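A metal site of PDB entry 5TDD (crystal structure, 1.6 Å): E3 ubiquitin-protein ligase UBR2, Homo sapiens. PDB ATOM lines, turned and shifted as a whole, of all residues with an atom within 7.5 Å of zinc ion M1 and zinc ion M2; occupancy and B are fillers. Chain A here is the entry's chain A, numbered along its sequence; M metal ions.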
ATOM      1  N   SER A   5     -36.539 -31.921 -22.000  1.00  0.00           N
ATOM      2  CA  SER A   5     -35.501 -32.648 -22.719  1.00  0.00           C
ATOM      3  C   SER A   5     -34.304 -32.897 -21.800  1.00  0.00           C
ATOM      4  O   SER A   5     -34.125 -32.225 -20.780  1.00  0.00           O
ATOM      5  CB  SER A   5     -35.061 -31.913 -23.989  1.00  0.00           C
ATOM      6  OG  SER A   5     -34.563 -30.616 -23.693  1.00  0.00           O
ATOM      7  N   LEU A   6     -33.467 -33.857 -22.205  1.00  0.00           N
ATOM      8  CA  LEU A   6     -32.228 -34.189 -21.524  1.00  0.00           C
ATOM      9  C   LEU A   6     -31.050 -33.479 -22.181  1.00  0.00           C
ATOM     10  O   LEU A   6     -30.954 -33.386 -23.416  1.00  0.00           O
ATOM     11  CB  LEU A   6     -31.976 -35.705 -21.545  1.00  0.00           C
ATOM     12  CG  LEU A   6     -32.979 -36.589 -20.800  1.00  0.00           C
ATOM     13  CD1 LEU A   6     -32.846 -38.015 -21.305  1.00  0.00           C
ATOM     14  CD2 LEU A   6     -32.720 -36.561 -19.338  1.00  0.00           C
ATOM     15  N   CYS A   7     -30.125 -32.986 -21.359  1.00  0.00           N
ATOM     16  CA  CYS A   7     -28.893 -32.417 -21.884  1.00  0.00           C
ATOM     17  C   CYS A   7     -27.961 -33.500 -22.387  1.00  0.00           C
ATOM     18  O   CYS A   7     -27.572 -33.498 -23.556  1.00  0.00           O
ATOM     19  CB  CYS A   7     -28.200 -31.583 -20.817  1.00  0.00           C
ATOM     20  SG  CYS A   7     -26.570 -30.884 -21.376  1.00  0.00           S
ATOM     21  N   GLY A   8     -27.523 -34.385 -21.498  1.00  0.00           N
ATOM     22  CA  GLY A   8     -26.659 -35.486 -21.857  1.00  0.00           C
ATOM     23  C   GLY A   8     -25.214 -35.171 -22.209  1.00  0.00           C
ATOM     24  O   GLY A   8     -24.494 -36.090 -22.622  1.00  0.00           O
ATOM     25  N   ARG A   9     -24.774 -33.922 -22.068  1.00  0.00           N
ATOM     26  CA  ARG A   9     -23.418 -33.531 -22.420  1.00  0.00           C
ATOM     27  C   ARG A   9     -22.375 -34.351 -21.658  1.00  0.00           C
ATOM     28  O   ARG A   9     -22.433 -34.428 -20.435  1.00  0.00           O
ATOM     29  CB  ARG A   9     -23.193 -32.053 -22.105  1.00  0.00           C
ATOM     30  CG  ARG A   9     -21.809 -31.591 -22.349  1.00  0.00           C
ATOM     31  CD  ARG A   9     -21.561 -30.141 -22.025  1.00  0.00           C
ATOM     32  NE  ARG A   9     -20.129 -29.866 -22.065  1.00  0.00           N
ATOM     33  CZ  ARG A   9     -19.433 -29.669 -23.182  1.00  0.00           C
ATOM     34  NH1 ARG A   9     -20.040 -29.680 -24.374  1.00  0.00           N
ATOM     35  NH2 ARG A   9     -18.125 -29.430 -23.104  1.00  0.00           N
ATOM     36  N   PHE A  11     -18.609 -34.613 -20.340  1.00  0.00           N
ATOM     37  CA  PHE A  11     -17.675 -33.596 -19.911  1.00  0.00           C
ATOM     38  C   PHE A  11     -16.282 -33.848 -20.477  1.00  0.00           C
ATOM     39  O   PHE A  11     -15.819 -34.987 -20.607  1.00  0.00           O
ATOM     40  CB  PHE A  11     -17.585 -33.525 -18.393  1.00  0.00           C
ATOM     41  CG  PHE A  11     -18.901 -33.241 -17.716  1.00  0.00           C
ATOM     42  CD1 PHE A  11     -19.554 -32.046 -17.912  1.00  0.00           C
ATOM     43  CD2 PHE A  11     -19.457 -34.161 -16.847  1.00  0.00           C
ATOM     44  CE1 PHE A  11     -20.750 -31.779 -17.262  1.00  0.00           C
ATOM     45  CE2 PHE A  11     -20.641 -33.889 -16.201  1.00  0.00           C
ATOM     46  CZ  PHE A  11     -21.294 -32.717 -16.404  1.00  0.00           C
ATOM     47  N   GLU A  15     -13.182 -29.954 -17.144  1.00  0.00           N
ATOM     48  CA  GLU A  15     -14.406 -29.149 -17.244  1.00  0.00           C
ATOM     49  C   GLU A  15     -15.117 -29.056 -15.897  1.00  0.00           C
ATOM     50  O   GLU A  15     -15.306 -30.083 -15.237  1.00  0.00           O
ATOM     51  CB  GLU A  15     -15.360 -29.757 -18.271  1.00  0.00           C
ATOM     52  CG  GLU A  15     -16.643 -28.967 -18.480  1.00  0.00           C
ATOM     53  CD  GLU A  15     -17.500 -29.437 -19.645  1.00  0.00           C
ATOM     54  OE1 GLU A  15     -16.998 -30.215 -20.484  1.00  0.00           O
ATOM     55  OE2 GLU A  15     -18.699 -29.015 -19.714  1.00  0.00           O
ATOM     56  N   VAL A  30     -25.014 -33.969 -11.385  1.00  0.00           N
ATOM     57  CA  VAL A  30     -24.306 -32.745 -11.754  1.00  0.00           C
ATOM     58  C   VAL A  30     -24.907 -32.119 -13.012  1.00  0.00           C
ATOM     59  O   VAL A  30     -25.592 -32.767 -13.797  1.00  0.00           O
ATOM     60  CB  VAL A  30     -22.786 -32.973 -11.980  1.00  0.00           C
ATOM     61  CG1 VAL A  30     -22.068 -33.234 -10.660  1.00  0.00           C
ATOM     62  CG2 VAL A  30     -22.579 -34.097 -12.934  1.00  0.00           C
ATOM     63  N   LEU A  31     -24.590 -30.837 -13.190  1.00  0.00           N
ATOM     64  CA  LEU A  31     -24.958 -30.057 -14.362  1.00  0.00           C
ATOM     65  C   LEU A  31     -23.710 -29.454 -14.999  1.00  0.00           C
ATOM     66  O   LEU A  31     -22.755 -29.092 -14.311  1.00  0.00           O
ATOM     67  CB  LEU A  31     -25.899 -28.905 -14.001  1.00  0.00           C
ATOM     68  CG  LEU A  31     -27.165 -29.279 -13.259  1.00  0.00           C
ATOM     69  CD1 LEU A  31     -27.847 -28.021 -12.739  1.00  0.00           C
ATOM     70  CD2 LEU A  31     -28.105 -30.055 -14.190  1.00  0.00           C
ATOM     71  N   CYS A  32     -23.697 -29.393 -16.313  1.00  0.00           N
ATOM     72  CA  CYS A  32     -22.702 -28.604 -17.010  1.00  0.00           C
ATOM     73  C   CYS A  32     -22.901 -27.121 -16.685  1.00  0.00           C
ATOM     74  O   CYS A  32     -23.956 -26.706 -16.196  1.00  0.00           O
ATOM     75  CB  CYS A  32     -22.778 -28.854 -18.526  1.00  0.00           C
ATOM     76  SG  CYS A  32     -24.289 -28.201 -19.376  1.00  0.00           S
ATOM     77  N   MET A  33     -21.886 -26.307 -16.975  1.00  0.00           N
ATOM     78  CA  MET A  33     -21.979 -24.898 -16.571  1.00  0.00           C
ATOM     79  C   MET A  33     -23.140 -24.189 -17.245  1.00  0.00           C
ATOM     80  O   MET A  33     -23.821 -23.390 -16.594  1.00  0.00           O
ATOM     81  CB  MET A  33     -20.677 -24.164 -16.846  1.00  0.00           C
ATOM     82  CG  MET A  33     -20.660 -22.749 -16.158  1.00  0.00           C
ATOM     83  SD  MET A  33     -19.164 -21.855 -16.568  1.00  0.00           S
ATOM     84  CE  MET A  33     -17.921 -22.848 -15.767  1.00  0.00           C
ATOM     85  N   GLU A  34     -23.404 -24.468 -18.533  1.00  0.00           N
ATOM     86  CA  GLU A  34     -24.513 -23.814 -19.222  1.00  0.00           C
ATOM     87  C   GLU A  34     -25.842 -24.118 -18.557  1.00  0.00           C
ATOM     88  O   GLU A  34     -26.660 -23.219 -18.335  1.00  0.00           O
ATOM     89  CB  GLU A  34     -24.550 -24.231 -20.691  1.00  0.00           C
ATOM     90  CG  GLU A  34     -25.667 -23.584 -21.470  1.00  0.00           C
ATOM     91  CD  GLU A  34     -25.603 -23.879 -22.961  1.00  0.00           C
ATOM     92  OE1 GLU A  34     -24.958 -24.878 -23.365  1.00  0.00           O
ATOM     93  OE2 GLU A  34     -26.206 -23.087 -23.713  1.00  0.00           O
ATOM     94  N   CYS A  35     -26.070 -25.385 -18.227  1.00  0.00           N
ATOM     95  CA  CYS A  35     -27.335 -25.762 -17.588  1.00  0.00           C
ATOM     96  C   CYS A  35     -27.409 -25.188 -16.178  1.00  0.00           C
ATOM     97  O   CYS A  35     -28.450 -24.645 -15.774  1.00  0.00           O
ATOM     98  CB  CYS A  35     -27.472 -27.281 -17.575  1.00  0.00           C
ATOM     99  SG  CYS A  35     -27.740 -27.994 -19.223  1.00  0.00           S
ATOM    100  N   PHE A  36     -26.292 -25.256 -15.444  1.00  0.00           N
ATOM    101  CA  PHE A  36     -26.238 -24.681 -14.107  1.00  0.00           C
ATOM    102  C   PHE A  36     -26.648 -23.214 -14.123  1.00  0.00           C
ATOM    103  O   PHE A  36     -27.498 -22.787 -13.322  1.00  0.00           O
ATOM    104  CB  PHE A  36     -24.802 -24.830 -13.543  1.00  0.00           C
ATOM    105  CG  PHE A  36     -24.576 -24.073 -12.277  1.00  0.00           C
ATOM    106  CD1 PHE A  36     -25.228 -24.426 -11.105  1.00  0.00           C
ATOM    107  CD2 PHE A  36     -23.699 -22.989 -12.250  1.00  0.00           C
ATOM    108  CE1 PHE A  36     -25.031 -23.717  -9.949  1.00  0.00           C
ATOM    109  CE2 PHE A  36     -23.490 -22.299 -11.105  1.00  0.00           C
ATOM    110  CZ  PHE A  36     -24.150 -22.664  -9.950  1.00  0.00           C
ATOM    111  N   GLY A  38     -28.363 -21.593 -16.204  1.00  0.00           N
ATOM    112  CA  GLY A  38     -29.758 -21.481 -16.585  1.00  0.00           C
ATOM    113  C   GLY A  38     -30.756 -22.145 -15.645  1.00  0.00           C
ATOM    114  O   GLY A  38     -31.937 -22.277 -15.990  1.00  0.00           O
ATOM    115  N   SER A  39     -30.318 -22.568 -14.472  1.00  0.00           N
ATOM    116  CA  SER A  39     -31.135 -23.346 -13.549  1.00  0.00           C
ATOM    117  C   SER A  39     -31.392 -22.579 -12.248  1.00  0.00           C
ATOM    118  O   SER A  39     -30.695 -21.625 -11.898  1.00  0.00           O
ATOM    119  CB  SER A  39     -30.464 -24.668 -13.214  1.00  0.00           C
ATOM    120  OG  SER A  39     -29.468 -24.531 -12.220  1.00  0.00           O
ATOM    121  N   PHE A  56     -21.318 -37.136 -17.294  1.00  0.00           N
ATOM    122  CA  PHE A  56     -22.269 -36.425 -18.145  1.00  0.00           C
ATOM    123  C   PHE A  56     -23.280 -35.620 -17.330  1.00  0.00           C
ATOM    124  O   PHE A  56     -23.531 -35.879 -16.157  1.00  0.00           O
ATOM    125  CB  PHE A  56     -22.975 -37.378 -19.139  1.00  0.00           C
ATOM    126  CG  PHE A  56     -23.892 -38.359 -18.484  1.00  0.00           C
ATOM    127  CD1 PHE A  56     -23.425 -39.606 -18.057  1.00  0.00           C
ATOM    128  CD2 PHE A  56     -25.238 -38.055 -18.312  1.00  0.00           C
ATOM    129  CE1 PHE A  56     -24.293 -40.527 -17.444  1.00  0.00           C
ATOM    130  CE2 PHE A  56     -26.102 -38.968 -17.702  1.00  0.00           C
ATOM    131  CZ  PHE A  56     -25.638 -40.192 -17.278  1.00  0.00           C
ATOM    132  N   CYS A  57     -23.810 -34.589 -17.979  1.00  0.00           N
ATOM    133  CA  CYS A  57     -24.777 -33.687 -17.377  1.00  0.00           C
ATOM    134  C   CYS A  57     -26.137 -34.373 -17.168  1.00  0.00           C
ATOM    135  O   CYS A  57     -26.672 -35.028 -18.072  1.00  0.00           O
ATOM    136  CB  CYS A  57     -24.949 -32.484 -18.308  1.00  0.00           C
ATOM    137  SG  CYS A  57     -26.150 -31.259 -17.676  1.00  0.00           S
ATOM    138  N   ASP A  58     -26.711 -34.170 -15.974  1.00  0.00           N
ATOM    139  CA  ASP A  58     -27.998 -34.777 -15.597  1.00  0.00           C
ATOM    140  C   ASP A  58     -29.165 -33.817 -15.735  1.00  0.00           C
ATOM    141  O   ASP A  58     -30.228 -34.068 -15.175  1.00  0.00           O
ATOM    142  CB  ASP A  58     -27.923 -35.298 -14.153  1.00  0.00           C
ATOM    143  CG  ASP A  58     -26.805 -36.317 -13.973  1.00  0.00           C
ATOM    144  OD1 ASP A  58     -26.843 -37.348 -14.682  1.00  0.00           O
ATOM    145  OD2 ASP A  58     -25.877 -36.086 -13.143  1.00  0.00           O
ATOM    146  N   CYS A  59     -28.997 -32.718 -16.494  1.00  0.00           N
ATOM    147  CA  CYS A  59     -30.112 -31.814 -16.699  1.00  0.00           C
ATOM    148  C   CYS A  59     -31.240 -32.550 -17.434  1.00  0.00           C
ATOM    149  O   CYS A  59     -30.997 -33.250 -18.429  1.00  0.00           O
ATOM    150  CB  CYS A  59     -29.641 -30.588 -17.468  1.00  0.00           C
ATOM    151  SG  CYS A  59     -30.908 -29.297 -17.517  1.00  0.00           S
ATOM    152  N   GLY A  60     -32.465 -32.389 -16.948  1.00  0.00           N
ATOM    153  CA  GLY A  60     -33.635 -33.060 -17.517  1.00  0.00           C
ATOM    154  C   GLY A  60     -33.981 -34.399 -16.896  1.00  0.00           C
ATOM    155  O   GLY A  60     -35.046 -34.958 -17.206  1.00  0.00           O
ATOM    156  N   PRO A  69     -35.347 -29.940 -12.100  1.00  0.00           N
ATOM    157  CA  PRO A  69     -34.592 -30.884 -12.925  1.00  0.00           C
ATOM    158  C   PRO A  69     -34.170 -30.322 -14.259  1.00  0.00           C
ATOM    159  O   PRO A  69     -33.239 -30.860 -14.854  1.00  0.00           O
ATOM    160  CB  PRO A  69     -35.541 -32.076 -13.105  1.00  0.00           C
ATOM    161  CG  PRO A  69     -36.872 -31.449 -12.975  1.00  0.00           C
ATOM    162  CD  PRO A  69     -36.743 -30.358 -11.964  1.00  0.00           C
ATOM    163  N   TYR A  70     -34.814 -29.266 -14.748  1.00  0.00           N
ATOM    164  CA  TYR A  70     -34.505 -28.677 -16.048  1.00  0.00           C
ATOM    165  C   TYR A  70     -33.950 -27.266 -15.877  1.00  0.00           C
ATOM    166  O   TYR A  70     -34.256 -26.566 -14.928  1.00  0.00           O
ATOM    167  CB  TYR A  70     -35.773 -28.583 -16.947  1.00  0.00           C
ATOM    168  CG  TYR A  70     -36.489 -29.876 -17.241  1.00  0.00           C
ATOM    169  CD1 TYR A  70     -37.546 -30.287 -16.471  1.00  0.00           C
ATOM    170  CD2 TYR A  70     -36.092 -30.672 -18.312  1.00  0.00           C
ATOM    171  CE1 TYR A  70     -38.200 -31.497 -16.732  1.00  0.00           C
ATOM    172  CE2 TYR A  70     -36.741 -31.889 -18.593  1.00  0.00           C
ATOM    173  CZ  TYR A  70     -37.788 -32.286 -17.797  1.00  0.00           C
ATOM    174  OH  TYR A  70     -38.429 -33.491 -18.061  1.00  0.00           O
ATOM    175  N   CYS A  71     -33.203 -26.841 -16.874  1.00  0.00           N
ATOM    176  CA  CYS A  71     -32.738 -25.466 -16.988  1.00  0.00           C
ATOM    177  C   CYS A  71     -33.552 -24.742 -18.073  1.00  0.00           C
ATOM    178  O   CYS A  71     -34.400 -25.328 -18.754  1.00  0.00           O
ATOM    179  CB  CYS A  71     -31.242 -25.414 -17.312  1.00  0.00           C
ATOM    180  SG  CYS A  71     -30.883 -25.813 -19.058  1.00  0.00           S
ATOM    181  N   GLN A  72     -33.284 -23.435 -18.221  1.00  0.00           N
ATOM    182  CA  GLN A  72     -34.032 -22.630 -19.189  1.00  0.00           C
ATOM    183  C   GLN A  72     -33.930 -23.192 -20.597  1.00  0.00           C
ATOM    184  O   GLN A  72     -34.873 -23.080 -21.380  1.00  0.00           O
ATOM    185  CB  GLN A  72     -33.489 -21.201 -19.184  1.00  0.00           C
ATOM    186  CG  GLN A  72     -33.742 -20.464 -17.911  1.00  0.00           C
ATOM    187  CD  GLN A  72     -33.304 -19.018 -18.039  1.00  0.00           C
ATOM    188  OE1 GLN A  72     -32.266 -18.725 -18.651  1.00  0.00           O
ATOM    189  NE2 GLN A  72     -34.116 -18.095 -17.478  1.00  0.00           N
ATOM    190  N   LYS A  73     -32.786 -23.779 -20.936  1.00  0.00           N
ATOM    191  CA  LYS A  73     -32.519 -24.288 -22.278  1.00  0.00           C
ATOM    192  C   LYS A  73     -33.242 -25.576 -22.562  1.00  0.00           C
ATOM    193  O   LYS A  73     -33.618 -25.814 -23.713  1.00  0.00           O
ATOM    194  CB  LYS A  73     -31.017 -24.530 -22.456  1.00  0.00           C
ATOM    195  CG  LYS A  73     -30.619 -25.044 -23.850  1.00  0.00           C
ATOM    196  CD  LYS A  73     -29.102 -25.154 -23.999  1.00  0.00           C
ATOM    197  CE  LYS A  73     -28.672 -25.346 -25.461  1.00  0.00           C
ATOM    198  NZ  LYS A  73     -27.303 -24.744 -25.733  1.00  0.00           N
ATOM    199  N   HIS A  74     -33.423 -26.422 -21.546  1.00  0.00           N
ATOM    200  CA  HIS A  74     -33.988 -27.768 -21.735  1.00  0.00           C
ATOM    201  C   HIS A  74     -35.421 -27.917 -21.266  1.00  0.00           C
ATOM    202  O   HIS A  74     -36.044 -28.953 -21.570  1.00  0.00           O
ATOM    203  CB  HIS A  74     -33.082 -28.808 -21.052  1.00  0.00           C
ATOM    204  CG  HIS A  74     -31.757 -28.932 -21.735  1.00  0.00           C
ATOM    205  ND1 HIS A  74     -30.557 -28.566 -21.159  1.00  0.00           N
ATOM    206  CD2 HIS A  74     -31.463 -29.309 -22.989  1.00  0.00           C
ATOM    207  CE1 HIS A  74     -29.585 -28.717 -22.032  1.00  0.00           C
ATOM    208  NE2 HIS A  74     -30.110 -29.199 -23.152  1.00  0.00           N
ATOM    209  N   GLU A  75     -35.985 -26.918 -20.601  1.00  0.00           N
ATOM    210  CA  GLU A  75     -37.361 -26.980 -20.138  1.00  0.00           C
ATOM    211  C   GLU A  75     -38.282 -27.084 -21.332  1.00  0.00           C
ATOM    212  O   GLU A  75     -39.349 -27.696 -21.185  1.00  0.00           O
ATOM    213  CB  GLU A  75     -37.718 -25.756 -19.267  1.00  0.00           C
ATOM    214  CG  GLU A  75     -37.840 -24.430 -20.019  1.00  0.00           C
ATOM    215  CD  GLU A  75     -38.043 -23.242 -19.066  1.00  0.00           C
ATOM    216  OE1 GLU A  75     -38.724 -23.467 -18.042  1.00  0.00           O
ATOM    217  OE2 GLU A  75     -37.553 -22.119 -19.324  1.00  0.00           O
HETATM  218 ZN    ZN M   1     -26.093 -29.708 -19.443  1.00  0.00          ZN
HETATM  219 ZN    ZN M   2     -30.103 -27.975 -19.237  1.00  0.00          ZN
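The backbone NH of Cys 7 is in hydrogen-bond range of the backbone carbonyl oxygen of Cys 59 (3.1 Å).
The backbone NH (N) of Cys 59 lies close to the side-chain sulfur (SG) of Cys 57 (3.4 Å).
N of Arg 9 lies close to SG of Cys 7 (3.6 Å).
The backbone NH (N) of Lys 73 sits close to the side-chain sulfur (SG) of Cys 71.
The backbone NH of Cys 57 sits at hydrogen-bond distance from the backbone carbonyl oxygen of Arg 9, 2.8 Å away.
N of Ser 5 lies within hydrogen-bond range of O of His 74, 3.0 Å away.
Of the 28 residues printed, 4 come within 4 Å of zinc ion M2.
Along chain A the residues within 4 Å of zinc ion M2 span positions 35 to 74.
The nearest printed residue that does not touch zinc ion M2 is Cys 7 (4.4 Å).
Of the 28 residues printed, 4 come within 4 Å of zinc ion M1.
The nearest printed residue that does not touch zinc ion M1 is Cys 59 (4.2 Å).
Zinc ion M2 is bound by ND1 of His 74 (2.1 Å), SG of Cys 71 (2.3 Å), SG of Cys 59 (2.3 Å) and SG of Cys 35 (2.4 Å).
SG of Cys 7 is bound to zinc ion M1 (2.3 Å).
The side-chain sulfur (SG) of Cys 32 is bound to zinc ion M1 (2.4 Å).
SG of Cys 57 binds zinc ion M1.
Zinc ion M1 is bound by SG of Cys 35 (2.4 Å).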
